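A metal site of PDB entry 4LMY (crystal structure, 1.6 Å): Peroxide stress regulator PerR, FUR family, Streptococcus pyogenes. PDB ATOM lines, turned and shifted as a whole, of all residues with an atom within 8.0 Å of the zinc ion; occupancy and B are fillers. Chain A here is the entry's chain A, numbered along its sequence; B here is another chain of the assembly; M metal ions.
Lys 109 touches the zinc ion (NZ to ZN, 3.8 Å). Along chain A the residues within 4 Å of the zinc ion span positions 104 to 147.
The side-chain sulfur (SG) of Cys 104 sits close to the backbone NH (N) of Ile 106, 3.5 Å away. O of Lys 109 sits at hydrogen-bond distance from OH of Tyr 131 of chain B (2.8 Å). The backbone carbonyl oxygen of Lys 109 lies within hydrogen-bond range of the backbone NH of Cys 104 (3.0 Å). The side-chain amino group of Lys 109 lies within salt-bridge range of the side-chain carboxylate of Asp 146, 3.999 Å away. The side-chain amino group of Lys 109 lies close to the side-chain sulfur of Cys 107 (3.0 Å). The side-chain sulfur of Cys 144 lies close to the backbone NH of Asp 146.
The zinc ion is bound by the side-chain sulfur of Cys 107 (2.3 Å), the side-chain sulfur of Cys 144 (2.3 Å), the side-chain sulfur of Cys 147 (2.4 Å) and the side-chain sulfur of Cys 104 (2.4 Å). The zinc ion has four donor atoms within binding distance.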
ATOM      1  N   VAL A 103       3.931 -14.163 -20.802  1.00  0.00           N
ATOM      2  CA  VAL A 103       4.950 -14.881 -21.567  1.00  0.00           C
ATOM      3  C   VAL A 103       5.689 -13.934 -22.513  1.00  0.00           C
ATOM      4  O   VAL A 103       5.071 -13.163 -23.230  1.00  0.00           O
ATOM      5  CB  VAL A 103       4.312 -16.020 -22.400  1.00  0.00           C
ATOM      6  CG1 VAL A 103       5.376 -16.760 -23.184  1.00  0.00           C
ATOM      7  CG2 VAL A 103       3.558 -16.978 -21.493  1.00  0.00           C
ATOM      8  N   CYS A 104       7.019 -13.977 -22.495  1.00  0.00           N
ATOM      9  CA  CYS A 104       7.778 -13.142 -23.406  1.00  0.00           C
ATOM     10  C   CYS A 104       7.659 -13.666 -24.839  1.00  0.00           C
ATOM     11  O   CYS A 104       7.899 -14.843 -25.106  1.00  0.00           O
ATOM     12  CB  CYS A 104       9.256 -13.068 -23.003  1.00  0.00           C
ATOM     13  SG  CYS A 104      10.210 -11.918 -24.030  1.00  0.00           S
ATOM     14  N   GLU A 105       7.267 -12.774 -25.743  1.00  0.00           N
ATOM     15  CA  GLU A 105       7.105 -13.123 -27.150  1.00  0.00           C
ATOM     16  C   GLU A 105       8.437 -13.533 -27.781  1.00  0.00           C
ATOM     17  O   GLU A 105       8.480 -14.346 -28.699  1.00  0.00           O
ATOM     18  CB  GLU A 105       6.533 -11.928 -27.916  1.00  0.00           C
ATOM     19  CG  GLU A 105       5.213 -11.404 -27.382  1.00  0.00           C
ATOM     20  CD  GLU A 105       4.020 -11.882 -28.181  1.00  0.00           C
ATOM     21  OE1 GLU A 105       3.043 -11.119 -28.300  1.00  0.00           O
ATOM     22  OE2 GLU A 105       4.053 -13.024 -28.686  1.00  0.00           O
ATOM     23  N   ILE A 106       9.523 -12.966 -27.267  1.00  0.00           N
ATOM     24  CA  ILE A 106      10.840 -13.182 -27.852  1.00  0.00           C
ATOM     25  C   ILE A 106      11.545 -14.416 -27.278  1.00  0.00           C
ATOM     26  O   ILE A 106      11.887 -15.341 -28.020  1.00  0.00           O
ATOM     27  CB  ILE A 106      11.727 -11.941 -27.715  1.00  0.00           C
ATOM     28  CG1 ILE A 106      11.074 -10.747 -28.423  1.00  0.00           C
ATOM     29  CG2 ILE A 106      13.128 -12.221 -28.276  1.00  0.00           C
ATOM     30  CD1 ILE A 106      11.889  -9.471 -28.379  1.00  0.00           C
ATOM     31  N   CYS A 107      11.765 -14.428 -25.965  1.00  0.00           N
ATOM     32  CA  CYS A 107      12.542 -15.513 -25.352  1.00  0.00           C
ATOM     33  C   CYS A 107      11.695 -16.608 -24.714  1.00  0.00           C
ATOM     34  O   CYS A 107      12.174 -17.713 -24.496  1.00  0.00           O
ATOM     35  CB  CYS A 107      13.548 -14.955 -24.338  1.00  0.00           C
ATOM     36  SG  CYS A 107      12.788 -14.379 -22.799  1.00  0.00           S
ATOM     37  N   GLY A 108      10.430 -16.309 -24.418  1.00  0.00           N
ATOM     38  CA  GLY A 108       9.530 -17.299 -23.866  1.00  0.00           C
ATOM     39  C   GLY A 108       9.557 -17.420 -22.352  1.00  0.00           C
ATOM     40  O   GLY A 108       8.832 -18.219 -21.778  1.00  0.00           O
ATOM     41  N   LYS A 109      10.395 -16.612 -21.693  1.00  0.00           N
ATOM     42  CA  LYS A 109      10.443 -16.638 -20.241  1.00  0.00           C
ATOM     43  C   LYS A 109       9.109 -16.189 -19.665  1.00  0.00           C
ATOM     44  O   LYS A 109       8.474 -15.270 -20.184  1.00  0.00           O
ATOM     45  CB  LYS A 109      11.586 -15.773 -19.715  1.00  0.00           C
ATOM     46  CG  LYS A 109      12.965 -16.342 -19.998  1.00  0.00           C
ATOM     47  CD  LYS A 109      14.070 -15.459 -19.432  1.00  0.00           C
ATOM     48  CE  LYS A 109      15.167 -15.143 -20.448  1.00  0.00           C
ATOM     49  NZ  LYS A 109      15.078 -13.745 -20.964  1.00  0.00           N
ATOM     50  N   ILE A 110       8.696 -16.854 -18.599  1.00  0.00           N
ATOM     51  CA  ILE A 110       7.390 -16.613 -18.005  1.00  0.00           C
ATOM     52  C   ILE A 110       7.497 -15.915 -16.654  1.00  0.00           C
ATOM     53  O   ILE A 110       8.299 -16.310 -15.805  1.00  0.00           O
ATOM     54  CB  ILE A 110       6.610 -17.934 -17.837  1.00  0.00           C
ATOM     55  CG1 ILE A 110       6.412 -18.607 -19.191  1.00  0.00           C
ATOM     56  CG2 ILE A 110       5.267 -17.681 -17.167  1.00  0.00           C
ATOM     57  CD1 ILE A 110       5.791 -19.980 -19.101  1.00  0.00           C
ATOM     58  N   GLY A 142       4.042 -10.394 -23.735  1.00  0.00           N
ATOM     59  CA  GLY A 142       4.742  -9.138 -23.807  1.00  0.00           C
ATOM     60  C   GLY A 142       6.218  -9.316 -24.069  1.00  0.00           C
ATOM     61  O   GLY A 142       6.654 -10.396 -24.464  1.00  0.00           O
ATOM     62  N   ILE A 143       6.988  -8.257 -23.848  1.00  0.00           N
ATOM     63  CA  ILE A 143       8.434  -8.314 -23.979  1.00  0.00           C
ATOM     64  C   ILE A 143       9.029  -8.158 -22.588  1.00  0.00           C
ATOM     65  O   ILE A 143       8.803  -7.161 -21.920  1.00  0.00           O
ATOM     66  CB  ILE A 143       8.960  -7.183 -24.872  1.00  0.00           C
ATOM     67  CG1 ILE A 143       8.175  -7.106 -26.191  1.00  0.00           C
ATOM     68  CG2 ILE A 143      10.447  -7.363 -25.143  1.00  0.00           C
ATOM     69  CD1 ILE A 143       8.302  -8.350 -27.046  1.00  0.00           C
ATOM     70  N   CYS A 144       9.781  -9.164 -22.157  1.00  0.00           N
ATOM     71  CA  CYS A 144      10.366  -9.143 -20.810  1.00  0.00           C
ATOM     72  C   CYS A 144      11.460  -8.073 -20.712  1.00  0.00           C
ATOM     73  O   CYS A 144      11.993  -7.631 -21.723  1.00  0.00           O
ATOM     74  CB  CYS A 144      10.927 -10.527 -20.450  1.00  0.00           C
ATOM     75  SG  CYS A 144      12.566 -10.893 -21.140  1.00  0.00           S
ATOM     76  N   PRO A 145      11.777  -7.639 -19.481  1.00  0.00           N
ATOM     77  CA  PRO A 145      12.785  -6.587 -19.293  1.00  0.00           C
ATOM     78  C   PRO A 145      14.117  -6.857 -19.996  1.00  0.00           C
ATOM     79  O   PRO A 145      14.732  -5.916 -20.507  1.00  0.00           O
ATOM     80  CB  PRO A 145      12.974  -6.579 -17.775  1.00  0.00           C
ATOM     81  CG  PRO A 145      11.640  -6.956 -17.253  1.00  0.00           C
ATOM     82  CD  PRO A 145      11.080  -7.967 -18.220  1.00  0.00           C
ATOM     83  N   ASP A 146      14.541  -8.117 -20.043  1.00  0.00           N
ATOM     84  CA  ASP A 146      15.800  -8.457 -20.687  1.00  0.00           C
ATOM     85  C   ASP A 146      15.748  -8.259 -22.200  1.00  0.00           C
ATOM     86  O   ASP A 146      16.725  -7.812 -22.802  1.00  0.00           O
ATOM     87  CB  ASP A 146      16.197  -9.907 -20.369  1.00  0.00           C
ATOM     88  CG  ASP A 146      16.848 -10.044 -19.011  1.00  0.00           C
ATOM     89  OD1 ASP A 146      17.381  -9.043 -18.494  1.00  0.00           O
ATOM     90  OD2 ASP A 146      16.834 -11.169 -18.459  1.00  0.00           O
ATOM     91  N   CYS A 147      14.607  -8.587 -22.805  1.00  0.00           N
ATOM     92  CA  CYS A 147      14.467  -8.511 -24.257  1.00  0.00           C
ATOM     93  C   CYS A 147      14.106  -7.121 -24.768  1.00  0.00           C
ATOM     94  O   CYS A 147      14.084  -6.884 -25.980  1.00  0.00           O
ATOM     95  CB  CYS A 147      13.451  -9.562 -24.748  1.00  0.00           C
ATOM     96  SG  CYS A 147      13.983 -11.283 -24.573  1.00  0.00           S
ATOM     97  N   GLN A 148      13.812  -6.201 -23.852  1.00  0.00           N
ATOM     98  CA  GLN A 148      13.475  -4.832 -24.227  1.00  0.00           C
ATOM     99  C   GLN A 148      14.710  -4.036 -24.670  1.00  0.00           C
ATOM    100  O   GLN A 148      15.785  -4.215 -24.103  1.00  0.00           O
ATOM    101  CB  GLN A 148      12.791  -4.111 -23.063  1.00  0.00           C
ATOM    102  CG  GLN A 148      11.370  -4.587 -22.787  1.00  0.00           C
ATOM    103  CD  GLN A 148      10.835  -4.093 -21.463  1.00  0.00           C
ATOM    104  OE1 GLN A 148      10.035  -4.779 -20.812  1.00  0.00           O
ATOM    105  NE2 GLN A 148      11.263  -2.910 -21.042  1.00  0.00           N
ATOM    106  N   TYR B 131       7.200  -6.386 -17.809  1.00  0.00           N
ATOM    107  CA  TYR B 131       6.981  -6.688 -19.228  1.00  0.00           C
ATOM    108  C   TYR B 131       6.245  -5.555 -19.935  1.00  0.00           C
ATOM    109  O   TYR B 131       5.328  -4.948 -19.374  1.00  0.00           O
ATOM    110  CB  TYR B 131       6.142  -7.958 -19.392  1.00  0.00           C
ATOM    111  CG  TYR B 131       6.862  -9.280 -19.198  1.00  0.00           C
ATOM    112  CD1 TYR B 131       6.756 -10.292 -20.148  1.00  0.00           C
ATOM    113  CD2 TYR B 131       7.624  -9.514 -18.069  1.00  0.00           C
ATOM    114  CE1 TYR B 131       7.380 -11.507 -19.968  1.00  0.00           C
ATOM    115  CE2 TYR B 131       8.270 -10.724 -17.886  1.00  0.00           C
ATOM    116  CZ  TYR B 131       8.151 -11.719 -18.844  1.00  0.00           C
ATOM    117  OH  TYR B 131       8.781 -12.922 -18.660  1.00  0.00           O
HETATM  118 ZN    ZN M   1      12.368 -12.135 -23.085  1.00  0.00          ZN
